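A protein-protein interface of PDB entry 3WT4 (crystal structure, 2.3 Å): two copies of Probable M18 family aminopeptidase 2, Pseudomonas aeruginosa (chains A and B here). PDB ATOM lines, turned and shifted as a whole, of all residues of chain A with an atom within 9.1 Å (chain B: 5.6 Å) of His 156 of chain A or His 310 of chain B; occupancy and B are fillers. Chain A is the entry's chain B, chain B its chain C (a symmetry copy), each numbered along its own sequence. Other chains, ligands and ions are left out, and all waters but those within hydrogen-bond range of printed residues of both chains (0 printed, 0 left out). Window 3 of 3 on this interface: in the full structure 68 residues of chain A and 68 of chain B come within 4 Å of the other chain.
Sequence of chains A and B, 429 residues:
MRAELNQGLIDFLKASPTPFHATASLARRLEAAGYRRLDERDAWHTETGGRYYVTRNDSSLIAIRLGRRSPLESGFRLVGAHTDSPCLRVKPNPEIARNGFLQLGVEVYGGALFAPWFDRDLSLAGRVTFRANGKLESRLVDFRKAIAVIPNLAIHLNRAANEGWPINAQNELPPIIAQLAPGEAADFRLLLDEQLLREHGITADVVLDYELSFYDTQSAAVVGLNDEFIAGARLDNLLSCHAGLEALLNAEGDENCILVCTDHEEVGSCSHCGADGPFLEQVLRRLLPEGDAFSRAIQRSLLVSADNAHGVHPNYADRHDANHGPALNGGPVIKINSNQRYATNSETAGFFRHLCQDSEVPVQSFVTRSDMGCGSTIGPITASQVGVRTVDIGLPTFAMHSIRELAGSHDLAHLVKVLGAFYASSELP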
ATOM      1  N   ASN A 152      35.267  22.282 -17.786  1.00  0.00           N
ATOM      2  CA  ASN A 152      34.554  23.026 -16.745  1.00  0.00           C
ATOM      3  C   ASN A 152      33.501  22.197 -16.052  1.00  0.00           C
ATOM      4  O   ASN A 152      33.053  21.215 -16.590  1.00  0.00           O
ATOM      5  CB  ASN A 152      33.957  24.293 -17.255  1.00  0.00           C
ATOM      6  CG  ASN A 152      34.881  25.493 -17.046  1.00  0.00           C
ATOM      7  OD1 ASN A 152      35.273  25.820 -15.933  1.00  0.00           O
ATOM      8  ND2 ASN A 152      35.241  26.134 -18.119  1.00  0.00           N
ATOM      9  N   LEU A 153      33.196  22.541 -14.807  1.00  0.00           N
ATOM     10  CA  LEU A 153      31.989  22.033 -14.147  1.00  0.00           C
ATOM     11  C   LEU A 153      30.797  22.796 -14.719  1.00  0.00           C
ATOM     12  O   LEU A 153      30.882  24.001 -14.870  1.00  0.00           O
ATOM     13  CB  LEU A 153      32.058  22.253 -12.609  1.00  0.00           C
ATOM     14  CG  LEU A 153      30.800  21.871 -11.822  1.00  0.00           C
ATOM     15  CD1 LEU A 153      30.463  20.377 -11.970  1.00  0.00           C
ATOM     16  CD2 LEU A 153      31.011  22.220 -10.352  1.00  0.00           C
ATOM     17  N   ALA A 154      29.707  22.115 -15.046  1.00  0.00           N
ATOM     18  CA  ALA A 154      28.502  22.784 -15.591  1.00  0.00           C
ATOM     19  C   ALA A 154      28.037  23.932 -14.686  1.00  0.00           C
ATOM     20  O   ALA A 154      28.077  23.806 -13.462  1.00  0.00           O
ATOM     21  CB  ALA A 154      27.349  21.784 -15.686  1.00  0.00           C
ATOM     22  N   ILE A 155      27.520  24.994 -15.273  1.00  0.00           N
ATOM     23  CA  ILE A 155      26.976  26.080 -14.475  1.00  0.00           C
ATOM     24  C   ILE A 155      25.827  25.634 -13.566  1.00  0.00           C
ATOM     25  O   ILE A 155      25.714  26.131 -12.433  1.00  0.00           O
ATOM     26  CB  ILE A 155      26.594  27.312 -15.314  1.00  0.00           C
ATOM     27  CG1 ILE A 155      26.330  28.531 -14.432  1.00  0.00           C
ATOM     28  CG2 ILE A 155      25.365  27.037 -16.181  1.00  0.00           C
ATOM     29  CD1 ILE A 155      26.262  29.832 -15.224  1.00  0.00           C
ATOM     30  N   HIS A 156      25.011  24.689 -14.058  1.00  0.00           N
ATOM     31  CA  HIS A 156      23.929  24.073 -13.290  1.00  0.00           C
ATOM     32  C   HIS A 156      24.367  23.544 -11.958  1.00  0.00           C
ATOM     33  O   HIS A 156      23.561  23.524 -11.069  1.00  0.00           O
ATOM     34  CB  HIS A 156      23.286  22.936 -14.028  1.00  0.00           C
ATOM     35  CG  HIS A 156      22.975  23.269 -15.449  1.00  0.00           C
ATOM     36  ND1 HIS A 156      23.959  23.419 -16.413  1.00  0.00           N
ATOM     37  CD2 HIS A 156      21.803  23.576 -16.051  1.00  0.00           C
ATOM     38  CE1 HIS A 156      23.399  23.780 -17.551  1.00  0.00           C
ATOM     39  NE2 HIS A 156      22.097  23.892 -17.355  1.00  0.00           N
ATOM     40  N   LEU A 157      25.625  23.143 -11.794  1.00  0.00           N
ATOM     41  CA  LEU A 157      26.135  22.565 -10.532  1.00  0.00           C
ATOM     42  C   LEU A 157      27.110  23.497  -9.827  1.00  0.00           C
ATOM     43  O   LEU A 157      27.828  23.085  -8.923  1.00  0.00           O
ATOM     44  CB  LEU A 157      26.895  21.282 -10.859  1.00  0.00           C
ATOM     45  CG  LEU A 157      26.051  20.210 -11.588  1.00  0.00           C
ATOM     46  CD1 LEU A 157      26.885  19.086 -12.128  1.00  0.00           C
ATOM     47  CD2 LEU A 157      25.024  19.634 -10.617  1.00  0.00           C
ATOM     48  N   ASN A 158      27.170  24.736 -10.297  1.00  0.00           N
ATOM     49  CA  ASN A 158      28.105  25.734  -9.805  1.00  0.00           C
ATOM     50  C   ASN A 158      27.465  27.054 -10.206  1.00  0.00           C
ATOM     51  O   ASN A 158      28.014  27.790 -10.992  1.00  0.00           O
ATOM     52  CB  ASN A 158      29.480  25.543 -10.480  1.00  0.00           C
ATOM     53  CG  ASN A 158      30.490  26.602 -10.066  1.00  0.00           C
ATOM     54  OD1 ASN A 158      30.311  27.291  -9.082  1.00  0.00           O
ATOM     55  ND2 ASN A 158      31.529  26.755 -10.846  1.00  0.00           N
ATOM     56  N   ARG A 159      26.260  27.290  -9.704  1.00  0.00           N
ATOM     57  CA  ARG A 159      25.368  28.388 -10.123  1.00  0.00           C
ATOM     58  C   ARG A 159      25.983  29.786 -10.019  1.00  0.00           C
ATOM     59  O   ARG A 159      25.626  30.674 -10.792  1.00  0.00           O
ATOM     60  CB  ARG A 159      24.104  28.390  -9.250  1.00  0.00           C
ATOM     61  CG  ARG A 159      23.111  27.291  -9.537  1.00  0.00           C
ATOM     62  CD  ARG A 159      22.070  27.789 -10.514  1.00  0.00           C
ATOM     63  NE  ARG A 159      21.246  26.677 -10.983  1.00  0.00           N
ATOM     64  CZ  ARG A 159      20.828  26.484 -12.241  1.00  0.00           C
ATOM     65  NH1 ARG A 159      21.148  27.335 -13.229  1.00  0.00           N
ATOM     66  NH2 ARG A 159      20.091  25.407 -12.516  1.00  0.00           N
ATOM     67  N   ALA A 160      26.856  30.008  -9.046  1.00  0.00           N
ATOM     68  CA  ALA A 160      27.556  31.291  -8.955  1.00  0.00           C
ATOM     69  C   ALA A 160      28.951  31.286  -9.655  1.00  0.00           C
ATOM     70  O   ALA A 160      29.764  32.167  -9.378  1.00  0.00           O
ATOM     71  CB  ALA A 160      27.642  31.758  -7.481  1.00  0.00           C
ATOM     72  N   ALA A 161      29.202  30.327 -10.559  1.00  0.00           N
ATOM     73  CA  ALA A 161      30.403  30.270 -11.385  1.00  0.00           C
ATOM     74  C   ALA A 161      30.923  31.598 -11.887  1.00  0.00           C
ATOM     75  O   ALA A 161      32.139  31.854 -11.813  1.00  0.00           O
ATOM     76  CB  ALA A 161      30.191  29.363 -12.604  1.00  0.00           C
ATOM     77  N   ASP B 236      24.635  21.002 -25.912  1.00  0.00           N
ATOM     78  CA  ASP B 236      23.371  21.339 -25.338  1.00  0.00           C
ATOM     79  C   ASP B 236      22.798  22.416 -26.229  1.00  0.00           C
ATOM     80  O   ASP B 236      23.223  23.575 -26.111  1.00  0.00           O
ATOM     81  CB  ASP B 236      23.540  21.863 -23.923  1.00  0.00           C
ATOM     82  CG  ASP B 236      22.261  22.475 -23.345  1.00  0.00           C
ATOM     83  OD1 ASP B 236      21.187  22.182 -23.866  1.00  0.00           O
ATOM     84  OD2 ASP B 236      22.344  23.282 -22.393  1.00  0.00           O
ATOM     85  N   GLU B 266      16.480  27.870 -23.287  1.00  0.00           N
ATOM     86  CA  GLU B 266      17.484  28.251 -22.349  1.00  0.00           C
ATOM     87  C   GLU B 266      17.010  29.436 -21.563  1.00  0.00           C
ATOM     88  O   GLU B 266      17.686  29.904 -20.664  1.00  0.00           O
ATOM     89  CB  GLU B 266      18.803  28.591 -23.064  1.00  0.00           C
ATOM     90  CG  GLU B 266      19.493  27.422 -23.731  1.00  0.00           C
ATOM     91  CD  GLU B 266      20.059  26.450 -22.730  1.00  0.00           C
ATOM     92  OE1 GLU B 266      19.842  26.650 -21.528  1.00  0.00           O
ATOM     93  OE2 GLU B 266      20.742  25.503 -23.138  1.00  0.00           O
ATOM     94  N   ASN B 308      20.679  17.310 -22.625  1.00  0.00           N
ATOM     95  CA  ASN B 308      21.899  16.754 -22.048  1.00  0.00           C
ATOM     96  C   ASN B 308      21.892  16.625 -20.503  1.00  0.00           C
ATOM     97  O   ASN B 308      21.385  17.481 -19.788  1.00  0.00           O
ATOM     98  CB  ASN B 308      23.144  17.492 -22.555  1.00  0.00           C
ATOM     99  CG  ASN B 308      23.334  17.364 -24.058  1.00  0.00           C
ATOM    100  OD1 ASN B 308      22.626  16.621 -24.744  1.00  0.00           O
ATOM    101  ND2 ASN B 308      24.278  18.120 -24.587  1.00  0.00           N
ATOM    102  N   ALA B 309      22.430  15.519 -20.020  1.00  0.00           N
ATOM    103  CA  ALA B 309      22.547  15.280 -18.605  1.00  0.00           C
ATOM    104  C   ALA B 309      23.982  15.622 -18.147  1.00  0.00           C
ATOM    105  O   ALA B 309      24.910  15.818 -18.979  1.00  0.00           O
ATOM    106  CB  ALA B 309      22.236  13.809 -18.306  1.00  0.00           C
ATOM    107  N   HIS B 310      24.144  15.688 -16.838  1.00  0.00           N
ATOM    108  CA  HIS B 310      25.451  15.903 -16.214  1.00  0.00           C
ATOM    109  C   HIS B 310      26.098  14.597 -15.852  1.00  0.00           C
ATOM    110  O   HIS B 310      25.652  13.859 -14.953  1.00  0.00           O
ATOM    111  CB  HIS B 310      25.295  16.685 -14.908  1.00  0.00           C
ATOM    112  CG  HIS B 310      24.637  17.984 -15.097  1.00  0.00           C
ATOM    113  ND1 HIS B 310      25.204  18.993 -15.837  1.00  0.00           N
ATOM    114  CD2 HIS B 310      23.425  18.437 -14.698  1.00  0.00           C
ATOM    115  CE1 HIS B 310      24.381  20.032 -15.864  1.00  0.00           C
ATOM    116  NE2 HIS B 310      23.304  19.728 -15.162  1.00  0.00           N
ATOM    117  N   GLY B 311      27.163  14.294 -16.541  1.00  0.00           N
ATOM    118  CA  GLY B 311      28.023  13.221 -16.116  1.00  0.00           C
ATOM    119  C   GLY B 311      28.736  13.600 -14.823  1.00  0.00           C
ATOM    120  O   GLY B 311      29.015  14.790 -14.556  1.00  0.00           O
ATOM    121  N   VAL B 312      29.049  12.597 -14.027  1.00  0.00           N
ATOM    122  CA  VAL B 312      29.929  12.856 -12.868  1.00  0.00           C
ATOM    123  C   VAL B 312      31.384  13.174 -13.279  1.00  0.00           C
ATOM    124  O   VAL B 312      32.084  12.391 -13.954  1.00  0.00           O
ATOM    125  CB  VAL B 312      29.836  11.775 -11.752  1.00  0.00           C
ATOM    126  CG1 VAL B 312      30.315  10.434 -12.241  1.00  0.00           C
ATOM    127  CG2 VAL B 312      30.635  12.256 -10.533  1.00  0.00           C
ATOM    128  N   HIS B 320      27.813  15.466  -7.533  1.00  0.00           N
ATOM    129  CA  HIS B 320      26.838  14.416  -7.793  1.00  0.00           C
ATOM    130  C   HIS B 320      26.509  13.617  -6.542  1.00  0.00           C
ATOM    131  O   HIS B 320      27.315  13.495  -5.633  1.00  0.00           O
ATOM    132  CB  HIS B 320      27.383  13.466  -8.861  1.00  0.00           C
ATOM    133  CG  HIS B 320      27.080  13.930 -10.234  1.00  0.00           C
ATOM    134  ND1 HIS B 320      27.710  15.027 -10.800  1.00  0.00           N
ATOM    135  CD2 HIS B 320      26.187  13.483 -11.148  1.00  0.00           C
ATOM    136  CE1 HIS B 320      27.225  15.219 -12.009  1.00  0.00           C
ATOM    137  NE2 HIS B 320      26.299  14.298 -12.239  1.00  0.00           N
ATOM    138  N   GLY B 325      25.822   9.004 -10.550  1.00  0.00           N
ATOM    139  CA  GLY B 325      26.813   9.711 -11.275  1.00  0.00           C
ATOM    140  C   GLY B 325      26.938   9.035 -12.604  1.00  0.00           C
ATOM    141  O   GLY B 325      27.490   7.988 -12.679  1.00  0.00           O
ATOM    142  N   PRO B 326      26.356   9.608 -13.644  1.00  0.00           N
ATOM    143  CA  PRO B 326      26.406   8.999 -14.979  1.00  0.00           C
ATOM    144  C   PRO B 326      27.797   9.106 -15.561  1.00  0.00           C
ATOM    145  O   PRO B 326      28.490  10.120 -15.360  1.00  0.00           O
ATOM    146  CB  PRO B 326      25.440   9.852 -15.787  1.00  0.00           C
ATOM    147  CG  PRO B 326      24.464  10.383 -14.786  1.00  0.00           C
ATOM    148  CD  PRO B 326      25.286  10.594 -13.525  1.00  0.00           C
ATOM    149  N   TYR B 342      12.068  17.668 -13.737  1.00  0.00           N
ATOM    150  CA  TYR B 342      11.947  16.691 -14.818  1.00  0.00           C
ATOM    151  C   TYR B 342      10.525  15.995 -14.660  1.00  0.00           C
ATOM    152  O   TYR B 342      10.030  15.836 -13.515  1.00  0.00           O
ATOM    153  CB  TYR B 342      13.104  15.632 -14.812  1.00  0.00           C
ATOM    154  CG  TYR B 342      14.566  16.128 -14.595  1.00  0.00           C
ATOM    155  CD1 TYR B 342      15.124  17.093 -15.400  1.00  0.00           C
ATOM    156  CD2 TYR B 342      15.392  15.571 -13.573  1.00  0.00           C
ATOM    157  CE1 TYR B 342      16.442  17.520 -15.204  1.00  0.00           C
ATOM    158  CE2 TYR B 342      16.714  15.996 -13.367  1.00  0.00           C
ATOM    159  CZ  TYR B 342      17.223  16.967 -14.185  1.00  0.00           C
ATOM    160  OH  TYR B 342      18.490  17.390 -14.043  1.00  0.00           O
ATOM    161  N   PHE B 366      19.782   9.527 -13.137  1.00  0.00           N
ATOM    162  CA  PHE B 366      20.249  10.752 -12.509  1.00  0.00           C
ATOM    163  C   PHE B 366      19.137  11.311 -11.661  1.00  0.00           C
ATOM    164  O   PHE B 366      17.985  11.525 -12.113  1.00  0.00           O
ATOM    165  CB  PHE B 366      20.628  11.828 -13.523  1.00  0.00           C
ATOM    166  CG  PHE B 366      21.054  13.139 -12.895  1.00  0.00           C
ATOM    167  CD1 PHE B 366      22.378  13.331 -12.447  1.00  0.00           C
ATOM    168  CD2 PHE B 366      20.149  14.168 -12.726  1.00  0.00           C
ATOM    169  CE1 PHE B 366      22.735  14.532 -11.840  1.00  0.00           C
ATOM    170  CE2 PHE B 366      20.517  15.377 -12.127  1.00  0.00           C
ATOM    171  CZ  PHE B 366      21.806  15.555 -11.678  1.00  0.00           C
ATOM    172  N   MET B 372      20.850  20.236  -3.400  1.00  0.00           N
ATOM    173  CA  MET B 372      21.016  21.128  -4.556  1.00  0.00           C
ATOM    174  C   MET B 372      19.735  21.090  -5.391  1.00  0.00           C
ATOM    175  O   MET B 372      19.139  20.018  -5.580  1.00  0.00           O
ATOM    176  CB  MET B 372      22.170  20.655  -5.480  1.00  0.00           C
ATOM    177  CG  MET B 372      23.596  20.715  -4.894  1.00  0.00           C
ATOM    178  SD  MET B 372      24.959  20.180  -6.002  1.00  0.00           S
ATOM    179  CE  MET B 372      25.344  21.731  -6.813  1.00  0.00           C
ATOM    180  N   LEU B 395      21.946  12.550 -22.857  1.00  0.00           N
ATOM    181  CA  LEU B 395      23.290  12.014 -22.881  1.00  0.00           C
ATOM    182  C   LEU B 395      24.165  12.761 -21.844  1.00  0.00           C
ATOM    183  O   LEU B 395      24.021  13.978 -21.665  1.00  0.00           O
ATOM    184  CB  LEU B 395      23.891  12.129 -24.262  1.00  0.00           C
ATOM    185  CG  LEU B 395      23.194  11.271 -25.305  1.00  0.00           C
ATOM    186  CD1 LEU B 395      24.013  11.394 -26.570  1.00  0.00           C
ATOM    187  CD2 LEU B 395      23.111   9.818 -24.843  1.00  0.00           C
ATOM    188  N   PRO B 396      25.050  12.041 -21.168  1.00  0.00           N
ATOM    189  CA  PRO B 396      25.886  12.609 -20.111  1.00  0.00           C
ATOM    190  C   PRO B 396      27.026  13.469 -20.659  1.00  0.00           C
ATOM    191  O   PRO B 396      27.788  13.073 -21.545  1.00  0.00           O
ATOM    192  CB  PRO B 396      26.383  11.361 -19.374  1.00  0.00           C
ATOM    193  CG  PRO B 396      26.395  10.309 -20.434  1.00  0.00           C
ATOM    194  CD  PRO B 396      25.182  10.587 -21.262  1.00  0.00           C
ATOM    195  N   THR B 397      27.101  14.686 -20.178  1.00  0.00           N
ATOM    196  CA  THR B 397      28.081  15.626 -20.678  1.00  0.00           C
ATOM    197  C   THR B 397      28.755  16.381 -19.544  1.00  0.00           C
ATOM    198  O   THR B 397      28.256  16.399 -18.407  1.00  0.00           O
ATOM    199  CB  THR B 397      27.399  16.657 -21.566  1.00  0.00           C
ATOM    200  OG1 THR B 397      26.493  17.441 -20.791  1.00  0.00           O
ATOM    201  CG2 THR B 397      26.699  16.003 -22.667  1.00  0.00           C
ATOM    202  N   MET B 400      28.550  21.984 -19.128  1.00  0.00           N
ATOM    203  CA  MET B 400      27.363  22.460 -19.789  1.00  0.00           C
ATOM    204  C   MET B 400      27.248  23.992 -19.620  1.00  0.00           C
ATOM    205  O   MET B 400      27.325  24.511 -18.482  1.00  0.00           O
ATOM    206  CB  MET B 400      26.117  21.807 -19.175  1.00  0.00           C
ATOM    207  CG  MET B 400      24.930  21.818 -20.159  1.00  0.00           C
ATOM    208  SD  MET B 400      23.509  20.768 -19.682  1.00  0.00           S
ATOM    209  CE  MET B 400      24.176  19.111 -19.450  1.00  0.00           C
ATOM    210  N   HIS B 401      26.973  24.652 -20.746  1.00  0.00           N
ATOM    211  CA  HIS B 401      26.853  26.091 -20.930  1.00  0.00           C
ATOM    212  C   HIS B 401      28.215  26.781 -21.134  1.00  0.00           C
ATOM    213  O   HIS B 401      28.286  27.982 -21.285  1.00  0.00           O
ATOM    214  CB  HIS B 401      25.983  26.750 -19.851  1.00  0.00           C
ATOM    215  CG  HIS B 401      24.528  26.410 -19.936  1.00  0.00           C
ATOM    216  ND1 HIS B 401      23.570  27.070 -19.199  1.00  0.00           N
ATOM    217  CD2 HIS B 401      23.857  25.497 -20.680  1.00  0.00           C
ATOM    218  CE1 HIS B 401      22.369  26.600 -19.516  1.00  0.00           C
ATOM    219  NE2 HIS B 401      22.515  25.661 -20.426  1.00  0.00           N
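His 310 of chain B touches Ala 154 of chain A (CE1 to CB, 3.5 Å). Ala 154 of chain A touches Met 400 of chain B. ND1 of His 401 of chain B touches CG2 of Ile 155 of chain A, 3.5 Å away. His 156 of chain A touches His 310 of chain B. His 156 of chain A touches Met 400 of chain B (CE1 to CG, 3.6 Å). His 156 of chain A touches His 401 of chain B (NE2 to CE1, 3.5 Å). Leu 157 of chain A touches His 310 of chain B (CD1 to CG, 3.9 Å). Leu 157 of chain A touches His 320 of chain B. O of Leu 157 of chain A touches CE of Met 372 of chain B, 3.5 Å away.
No position is printed for both chains.
NE2 of His 320 of chain B is in hydrogen-bond range of O of His 310 of chain B, 2.8 Å away.
N of Ile 155 of chain A lies within hydrogen-bond range of O of Met 400 of chain B (3.3 Å).
Of the printed residues of chain B, Ile 155 of chain A touches Met 400 and His 401. Ala 161 of chain A touches none of the printed residues of chain B. No residue of chain A comes within 4 Å of Ala 309 of chain B. His 310 of chain B touches three residues of chain A. Val 312 of chain B touches none of the printed residues of chain A. Of the printed residues of chain A, His 320 of chain B touches Leu 157.
Printed residues of chain B that touch a printed residue of chain A: His 310, His 320, Met 372, Met 400 and His 401. Of the 10 printed residues of chain A, 4 touch a printed residue of chain B. Hydrophobic or aromatic side chains of chain A within 4 Å of the printed part of chain B: Ala 154, Ile 155, His 156 and Leu 157. Among the printed residues, no Asp or Glu carboxylate lies within 4 Å of a Lys or Arg side-chain nitrogen of the other chain.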
